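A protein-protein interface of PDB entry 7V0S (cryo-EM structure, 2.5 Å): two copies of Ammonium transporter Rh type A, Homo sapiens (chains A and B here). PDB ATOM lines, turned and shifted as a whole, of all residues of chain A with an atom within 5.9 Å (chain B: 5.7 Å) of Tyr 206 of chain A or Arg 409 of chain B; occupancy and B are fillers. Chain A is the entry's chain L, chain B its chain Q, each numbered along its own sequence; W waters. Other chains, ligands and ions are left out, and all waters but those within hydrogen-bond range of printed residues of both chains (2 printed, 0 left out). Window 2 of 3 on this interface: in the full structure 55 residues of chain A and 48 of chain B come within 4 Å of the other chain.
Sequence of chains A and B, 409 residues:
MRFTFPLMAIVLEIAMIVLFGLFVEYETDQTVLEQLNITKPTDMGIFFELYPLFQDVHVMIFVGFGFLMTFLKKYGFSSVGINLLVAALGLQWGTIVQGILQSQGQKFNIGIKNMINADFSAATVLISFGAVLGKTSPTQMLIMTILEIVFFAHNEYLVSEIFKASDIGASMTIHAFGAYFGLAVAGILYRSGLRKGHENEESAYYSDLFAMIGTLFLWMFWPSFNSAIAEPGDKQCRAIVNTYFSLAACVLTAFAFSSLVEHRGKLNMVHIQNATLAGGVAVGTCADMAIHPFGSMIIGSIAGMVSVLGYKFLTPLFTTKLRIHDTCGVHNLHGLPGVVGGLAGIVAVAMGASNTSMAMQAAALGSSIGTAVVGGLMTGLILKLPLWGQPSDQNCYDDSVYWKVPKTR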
ATOM      1  N   ALA A 204      14.468  11.405  -2.831  1.00  0.00           N
ATOM      2  CA  ALA A 204      14.135  10.814  -1.546  1.00  0.00           C
ATOM      3  C   ALA A 204      13.539  11.889  -0.652  1.00  0.00           C
ATOM      4  O   ALA A 204      13.529  13.074  -0.995  1.00  0.00           O
ATOM      5  CB  ALA A 204      15.358  10.173  -0.876  1.00  0.00           C
ATOM      6  N   TYR A 205      13.035  11.460   0.504  1.00  0.00           N
ATOM      7  CA  TYR A 205      12.372  12.379   1.424  1.00  0.00           C
ATOM      8  C   TYR A 205      13.362  13.383   2.010  1.00  0.00           C
ATOM      9  O   TYR A 205      13.194  14.607   1.880  1.00  0.00           O
ATOM     10  CB  TYR A 205      11.679  11.573   2.526  1.00  0.00           C
ATOM     11  CG  TYR A 205      10.763  12.385   3.399  1.00  0.00           C
ATOM     12  CD1 TYR A 205       9.651  13.019   2.866  1.00  0.00           C
ATOM     13  CD2 TYR A 205      11.011  12.525   4.756  1.00  0.00           C
ATOM     14  CE1 TYR A 205       8.817  13.768   3.655  1.00  0.00           C
ATOM     15  CE2 TYR A 205      10.178  13.274   5.555  1.00  0.00           C
ATOM     16  CZ  TYR A 205       9.082  13.893   4.998  1.00  0.00           C
ATOM     17  OH  TYR A 205       8.247  14.643   5.785  1.00  0.00           O
ATOM     18  N   TYR A 206      14.416  12.880   2.653  1.00  0.00           N
ATOM     19  CA  TYR A 206      15.413  13.770   3.234  1.00  0.00           C
ATOM     20  C   TYR A 206      16.216  14.487   2.158  1.00  0.00           C
ATOM     21  O   TYR A 206      16.721  15.587   2.398  1.00  0.00           O
ATOM     22  CB  TYR A 206      16.335  12.989   4.163  1.00  0.00           C
ATOM     23  CG  TYR A 206      15.628  12.380   5.346  1.00  0.00           C
ATOM     24  CD1 TYR A 206      14.571  13.036   5.962  1.00  0.00           C
ATOM     25  CD2 TYR A 206      16.017  11.146   5.847  1.00  0.00           C
ATOM     26  CE1 TYR A 206      13.924  12.482   7.043  1.00  0.00           C
ATOM     27  CE2 TYR A 206      15.376  10.585   6.930  1.00  0.00           C
ATOM     28  CZ  TYR A 206      14.330  11.257   7.524  1.00  0.00           C
ATOM     29  OH  TYR A 206      13.689  10.700   8.603  1.00  0.00           O
ATOM     30  N   SER A 207      16.337  13.890   0.972  1.00  0.00           N
ATOM     31  CA  SER A 207      16.989  14.576  -0.138  1.00  0.00           C
ATOM     32  C   SER A 207      16.226  15.833  -0.537  1.00  0.00           C
ATOM     33  O   SER A 207      16.828  16.885  -0.781  1.00  0.00           O
ATOM     34  CB  SER A 207      17.123  13.628  -1.328  1.00  0.00           C
ATOM     35  OG  SER A 207      18.106  12.641  -1.087  1.00  0.00           O
ATOM     36  N   ASP A 208      14.894  15.748  -0.599  1.00  0.00           N
ATOM     37  CA  ASP A 208      14.096  16.931  -0.904  1.00  0.00           C
ATOM     38  C   ASP A 208      14.141  17.931   0.244  1.00  0.00           C
ATOM     39  O   ASP A 208      14.131  19.150   0.022  1.00  0.00           O
ATOM     40  CB  ASP A 208      12.658  16.526  -1.223  1.00  0.00           C
ATOM     41  CG  ASP A 208      12.529  15.857  -2.577  1.00  0.00           C
ATOM     42  OD1 ASP A 208      11.624  15.017  -2.746  1.00  0.00           O
ATOM     43  OD2 ASP A 208      13.337  16.169  -3.475  1.00  0.00           O
ATOM     44  N   LEU A 209      14.210  17.432   1.483  1.00  0.00           N
ATOM     45  CA  LEU A 209      14.412  18.329   2.618  1.00  0.00           C
ATOM     46  C   LEU A 209      15.718  19.109   2.482  1.00  0.00           C
ATOM     47  O   LEU A 209      15.770  20.307   2.783  1.00  0.00           O
ATOM     48  CB  LEU A 209      14.392  17.535   3.921  1.00  0.00           C
ATOM     49  CG  LEU A 209      14.545  18.316   5.226  1.00  0.00           C
ATOM     50  CD1 LEU A 209      13.500  19.415   5.329  1.00  0.00           C
ATOM     51  CD2 LEU A 209      14.458  17.376   6.415  1.00  0.00           C
ATOM     52  N   PHE A 210      16.785  18.444   2.034  1.00  0.00           N
ATOM     53  CA  PHE A 210      18.059  19.127   1.830  1.00  0.00           C
ATOM     54  C   PHE A 210      17.995  20.091   0.652  1.00  0.00           C
ATOM     55  O   PHE A 210      18.637  21.147   0.671  1.00  0.00           O
ATOM     56  CB  PHE A 210      19.177  18.103   1.627  1.00  0.00           C
ATOM     57  CG  PHE A 210      19.918  17.764   2.883  1.00  0.00           C
ATOM     58  CD1 PHE A 210      21.008  18.516   3.281  1.00  0.00           C
ATOM     59  CD2 PHE A 210      19.520  16.699   3.673  1.00  0.00           C
ATOM     60  CE1 PHE A 210      21.688  18.212   4.440  1.00  0.00           C
ATOM     61  CE2 PHE A 210      20.197  16.389   4.831  1.00  0.00           C
ATOM     62  CZ  PHE A 210      21.284  17.146   5.213  1.00  0.00           C
ATOM     63  N   ALA A 211      17.239  19.739  -0.390  1.00  0.00           N
ATOM     64  CA  ALA A 211      17.090  20.637  -1.534  1.00  0.00           C
ATOM     65  C   ALA A 211      16.352  21.916  -1.154  1.00  0.00           C
ATOM     66  O   ALA A 211      16.593  22.980  -1.747  1.00  0.00           O
ATOM     67  CB  ALA A 211      16.370  19.919  -2.673  1.00  0.00           C
ATOM     68  N   THR A 408      25.346   3.385   5.263  1.00  0.00           N
ATOM     69  CA  THR A 408      23.991   3.695   5.693  1.00  0.00           C
ATOM     70  C   THR A 408      23.669   5.138   5.333  1.00  0.00           C
ATOM     71  O   THR A 408      24.561   5.968   5.138  1.00  0.00           O
ATOM     72  CB  THR A 408      23.800   3.473   7.202  1.00  0.00           C
ATOM     73  OG1 THR A 408      24.614   4.396   7.934  1.00  0.00           O
ATOM     74  CG2 THR A 408      24.171   2.050   7.596  1.00  0.00           C
ATOM     75  N   ARG A 409      22.377   5.431   5.248  1.00  0.00           N
ATOM     76  CA  ARG A 409      21.904   6.763   4.892  1.00  0.00           C
ATOM     77  C   ARG A 409      21.856   7.687   6.107  1.00  0.00           C
ATOM     78  O   ARG A 409      22.123   8.883   6.006  1.00  0.00           O
ATOM     79  CB  ARG A 409      20.521   6.679   4.245  1.00  0.00           C
ATOM     80  CG  ARG A 409      20.411   5.639   3.146  1.00  0.00           C
ATOM     81  CD  ARG A 409      20.822   6.208   1.806  1.00  0.00           C
ATOM     82  NE  ARG A 409      19.885   7.224   1.342  1.00  0.00           N
ATOM     83  CZ  ARG A 409      20.023   7.912   0.218  1.00  0.00           C
ATOM     84  NH1 ARG A 409      21.051   7.717  -0.589  1.00  0.00           N
ATOM     85  NH2 ARG A 409      19.108   8.821  -0.101  1.00  0.00           N
ATOM     86  OXT ARG A 409      21.548   7.262   7.219  1.00  0.00           O
ATOM     87  N   LYS B  73      27.822   9.360  12.384  1.00  0.00           N
ATOM     88  CA  LYS B  73      26.455   8.913  12.132  1.00  0.00           C
ATOM     89  C   LYS B  73      25.603   8.930  13.397  1.00  0.00           C
ATOM     90  O   LYS B  73      24.381   9.092  13.313  1.00  0.00           O
ATOM     91  CB  LYS B  73      26.450   7.514  11.511  1.00  0.00           C
ATOM     92  CG  LYS B  73      26.623   6.376  12.506  1.00  0.00           C
ATOM     93  CD  LYS B  73      26.706   5.025  11.832  1.00  0.00           C
ATOM     94  CE  LYS B  73      27.718   4.130  12.525  1.00  0.00           C
ATOM     95  NZ  LYS B  73      27.237   3.637  13.842  1.00  0.00           N
ATOM     96  N   LYS B  74      26.215   8.768  14.570  1.00  0.00           N
ATOM     97  CA  LYS B  74      25.482   8.738  15.829  1.00  0.00           C
ATOM     98  C   LYS B  74      25.892   9.863  16.769  1.00  0.00           C
ATOM     99  O   LYS B  74      25.632   9.782  17.971  1.00  0.00           O
ATOM    100  CB  LYS B  74      25.667   7.392  16.528  1.00  0.00           C
ATOM    101  CG  LYS B  74      25.085   6.204  15.794  1.00  0.00           C
ATOM    102  CD  LYS B  74      25.589   4.906  16.392  1.00  0.00           C
ATOM    103  CE  LYS B  74      24.486   4.178  17.144  1.00  0.00           C
ATOM    104  NZ  LYS B  74      24.968   3.624  18.440  1.00  0.00           N
ATOM    105  N   ALA B 204      27.674   8.765   7.658  1.00  0.00           N
ATOM    106  CA  ALA B 204      26.495   8.348   6.917  1.00  0.00           C
ATOM    107  C   ALA B 204      26.206   9.394   5.847  1.00  0.00           C
ATOM    108  O   ALA B 204      26.787  10.480   5.844  1.00  0.00           O
ATOM    109  CB  ALA B 204      25.280   8.155   7.833  1.00  0.00           C
ATOM    110  N   TYR B 205      25.299   9.046   4.934  1.00  0.00           N
ATOM    111  CA  TYR B 205      25.032   9.870   3.756  1.00  0.00           C
ATOM    112  C   TYR B 205      24.525  11.263   4.135  1.00  0.00           C
ATOM    113  O   TYR B 205      25.108  12.287   3.750  1.00  0.00           O
ATOM    114  CB  TYR B 205      24.024   9.133   2.869  1.00  0.00           C
ATOM    115  CG  TYR B 205      23.646   9.829   1.588  1.00  0.00           C
ATOM    116  CD1 TYR B 205      24.486   9.797   0.482  1.00  0.00           C
ATOM    117  CD2 TYR B 205      22.437  10.499   1.474  1.00  0.00           C
ATOM    118  CE1 TYR B 205      24.135  10.426  -0.693  1.00  0.00           C
ATOM    119  CE2 TYR B 205      22.081  11.129   0.307  1.00  0.00           C
ATOM    120  CZ  TYR B 205      22.932  11.091  -0.774  1.00  0.00           C
ATOM    121  OH  TYR B 205      22.572  11.719  -1.938  1.00  0.00           O
ATOM    122  N   TYR B 206      23.457  11.317   4.928  1.00  0.00           N
ATOM    123  CA  TYR B 206      22.877  12.606   5.285  1.00  0.00           C
ATOM    124  C   TYR B 206      23.718  13.329   6.327  1.00  0.00           C
ATOM    125  O   TYR B 206      23.744  14.567   6.353  1.00  0.00           O
ATOM    126  CB  TYR B 206      21.440  12.410   5.764  1.00  0.00           C
ATOM    127  CG  TYR B 206      20.513  11.980   4.653  1.00  0.00           C
ATOM    128  CD1 TYR B 206      20.317  12.786   3.539  1.00  0.00           C
ATOM    129  CD2 TYR B 206      19.849  10.762   4.705  1.00  0.00           C
ATOM    130  CE1 TYR B 206      19.479  12.397   2.516  1.00  0.00           C
ATOM    131  CE2 TYR B 206      19.007  10.366   3.687  1.00  0.00           C
ATOM    132  CZ  TYR B 206      18.826  11.186   2.594  1.00  0.00           C
ATOM    133  OH  TYR B 206      17.990  10.798   1.576  1.00  0.00           O
ATOM    134  N   SER B 207      24.427  12.582   7.174  1.00  0.00           N
ATOM    135  CA  SER B 207      25.406  13.199   8.062  1.00  0.00           C
ATOM    136  C   SER B 207      26.497  13.896   7.262  1.00  0.00           C
ATOM    137  O   SER B 207      26.927  15.002   7.610  1.00  0.00           O
ATOM    138  CB  SER B 207      26.007  12.148   8.995  1.00  0.00           C
ATOM    139  OG  SER B 207      25.004  11.493   9.747  1.00  0.00           O
ATOM    140  N   PRO B 406      15.969  10.174  18.850  1.00  0.00           N
ATOM    141  CA  PRO B 406      14.742   9.592  18.298  1.00  0.00           C
ATOM    142  C   PRO B 406      14.979   8.186  17.770  1.00  0.00           C
ATOM    143  O   PRO B 406      16.069   7.844  17.307  1.00  0.00           O
ATOM    144  CB  PRO B 406      14.371  10.556  17.164  1.00  0.00           C
ATOM    145  CG  PRO B 406      15.077  11.824  17.489  1.00  0.00           C
ATOM    146  CD  PRO B 406      16.339  11.429  18.178  1.00  0.00           C
ATOM    147  N   LYS B 407      13.932   7.362  17.860  1.00  0.00           N
ATOM    148  CA  LYS B 407      14.013   5.997  17.351  1.00  0.00           C
ATOM    149  C   LYS B 407      14.240   5.986  15.845  1.00  0.00           C
ATOM    150  O   LYS B 407      15.024   5.179  15.333  1.00  0.00           O
ATOM    151  CB  LYS B 407      12.738   5.234  17.715  1.00  0.00           C
ATOM    152  CG  LYS B 407      12.459   4.011  16.857  1.00  0.00           C
ATOM    153  CD  LYS B 407      10.998   3.950  16.446  1.00  0.00           C
ATOM    154  CE  LYS B 407      10.142   3.334  17.540  1.00  0.00           C
ATOM    155  NZ  LYS B 407       8.735   3.138  17.097  1.00  0.00           N
ATOM    156  N   THR B 408      13.581   6.889  15.126  1.00  0.00           N
ATOM    157  CA  THR B 408      13.689   6.972  13.678  1.00  0.00           C
ATOM    158  C   THR B 408      14.875   7.841  13.279  1.00  0.00           C
ATOM    159  O   THR B 408      15.089   8.920  13.839  1.00  0.00           O
ATOM    160  CB  THR B 408      12.398   7.544  13.082  1.00  0.00           C
ATOM    161  OG1 THR B 408      11.290   6.714  13.449  1.00  0.00           O
ATOM    162  CG2 THR B 408      12.481   7.617  11.568  1.00  0.00           C
ATOM    163  N   ARG B 409      15.646   7.364  12.311  1.00  0.00           N
ATOM    164  CA  ARG B 409      16.722   8.159  11.735  1.00  0.00           C
ATOM    165  C   ARG B 409      16.161   9.238  10.808  1.00  0.00           C
ATOM    166  O   ARG B 409      16.533  10.407  10.893  1.00  0.00           O
ATOM    167  CB  ARG B 409      17.700   7.267  10.975  1.00  0.00           C
ATOM    168  CG  ARG B 409      18.630   8.027  10.052  1.00  0.00           C
ATOM    169  CD  ARG B 409      20.079   7.743  10.368  1.00  0.00           C
ATOM    170  NE  ARG B 409      20.966   8.482   9.480  1.00  0.00           N
ATOM    171  CZ  ARG B 409      21.839   9.393   9.885  1.00  0.00           C
ATOM    172  NH1 ARG B 409      21.982   9.693  11.165  1.00  0.00           N
ATOM    173  NH2 ARG B 409      22.587  10.020   8.981  1.00  0.00           N
ATOM    174  OXT ARG B 409      15.314   8.969   9.956  1.00  0.00           O
HETATM  175  O   HOH W   1      20.356  13.679  -1.832  1.00  0.00           O
HETATM  176  O   HOH W   2      14.986   9.855   2.750  1.00  0.00           O
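OH of Tyr 206 of chain A is in hydrogen-bond range of OXT of Arg 409 of chain B, at 2.7 Å. OG of Ser 207 of chain A sits at hydrogen-bond distance from OH of Tyr 206 of chain B, at 3.2 Å. O of Thr 408 of chain A lies within hydrogen-bond range of N of Tyr 205 of chain B (3.2 Å). The backbone NH (N) of Tyr 205 of chain B sits at hydrogen-bond distance from the chain-end carboxylate (O) of Arg 409 of chain A, 3.4 Å away. NH2 of Arg 409 of chain A is in hydrogen-bond range of OH of Tyr 206 of chain B. OXT of Arg 409 of chain A is in salt-bridge range of NE of Arg 409 of chain B (2.6 Å).
The guanidinium group (NH1) of Arg 409 of chain B sits at hydrogen-bond distance from the backbone carbonyl oxygen (O) of Lys 73 of chain B (3.3 Å). The guanidinium group (NH2) of Arg 409 of chain B sits at hydrogen-bond distance from the side-chain hydroxyl (OG) of Ser 207 of chain B (2.9 Å).
Ala 204 of chain A touches Tyr 206 of chain B (CB to OH, 3.7 Å). CZ of Tyr 206 of chain B touches CB of Tyr 206 of chain A, at 3.5 Å. Tyr 206 of chain B touches Phe 210 of chain A. O of Thr 408 of chain A touches CB of Ala 204 of chain B (3.5 Å). Ala 204 of chain B touches Arg 409 of chain A.
Of the printed residues of chain B, Tyr 206 of chain A touches Tyr 206 and Arg 409. Of the printed residues of chain B, Phe 210 of chain A touches Tyr 206. Of the printed residues of chain B, Thr 408 of chain A touches Ala 204 (3.5 Å) and Tyr 205 (3.2 Å). Printed residues of chain B within 4 Å of Arg 409 of chain A: Ala 204 (3.7 Å), Tyr 205 (3.4 Å), Tyr 206 (2.8 Å) and Arg 409 (2.6 Å). Lys 73 of chain B touches none of the printed residues of chain A. Lys 74 of chain B touches none of the printed residues of chain A. Printed residues of chain A within 4 Å of Ala 204 of chain B: Thr 408 and Arg 409. Of the printed residues of chain A, Tyr 206 of chain B touches Ala 204 (3.7 Å), Tyr 206 (3.5 Å), Ser 207 (3.2 Å), Phe 210 (3.7 Å) and Arg 409 (2.8 Å). Arg 409 of chain B touches just these residues of chain A: Tyr 206 and Arg 409.
Of the 10 printed residues of chain A, 6 touch a printed residue of chain B. Hydrophobic or aromatic side chains of chain A that line the printed part of chain B: Ala 204, Tyr 206 and Phe 210. Of the 10 printed residues of chain B, 4 touch a printed residue of chain A. Printed residues of chain B that touch a printed residue of chain A: Ala 204, Tyr 205, Tyr 206 and Arg 409. Hydrophobic or aromatic side chains of chain B within 4 Å of the printed part of chain A: Ala 204, Tyr 205 and Tyr 206. Along chain B the printed residues that touch a printed residue of chain A span positions 204 to 409.
Ala 204 of chain A touches Tyr 206 of chain B, but with the chains exchanged Tyr 206 of chain A does not touch Ala 204 of chain B (9.9 Å). Tyr 206 of chain B touches its own counterpart, Tyr 206 of chain A. Tyr 206 of chain A touches Arg 409 of chain B, and with the chains exchanged Arg 409 of chain A touches Tyr 206 of chain B. Ser 207 of chain A touches Tyr 206 of chain B, but with the chains exchanged Tyr 206 of chain A does not touch Ser 207 of chain B (8.6 Å). Positions printed for both chains: 204, 205, 206, 207, 408 and 409. Of the 11 pairs that touch across the chains among the printed residues, 4 have their exchanged pair printed and touching as well.
Water W1 bridges the side-chain hydroxyl of Ser 207 of chain A and the side-chain hydroxyl of Tyr 205 of chain B. Water W2 lies within hydrogen-bond range of the backbone NH of Tyr 206 of chain A (3.1 Å), the side-chain hydroxyl of Tyr 206 of chain B (3.4 Å) and the backbone NH of Tyr 205 of chain A (3.4 Å).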
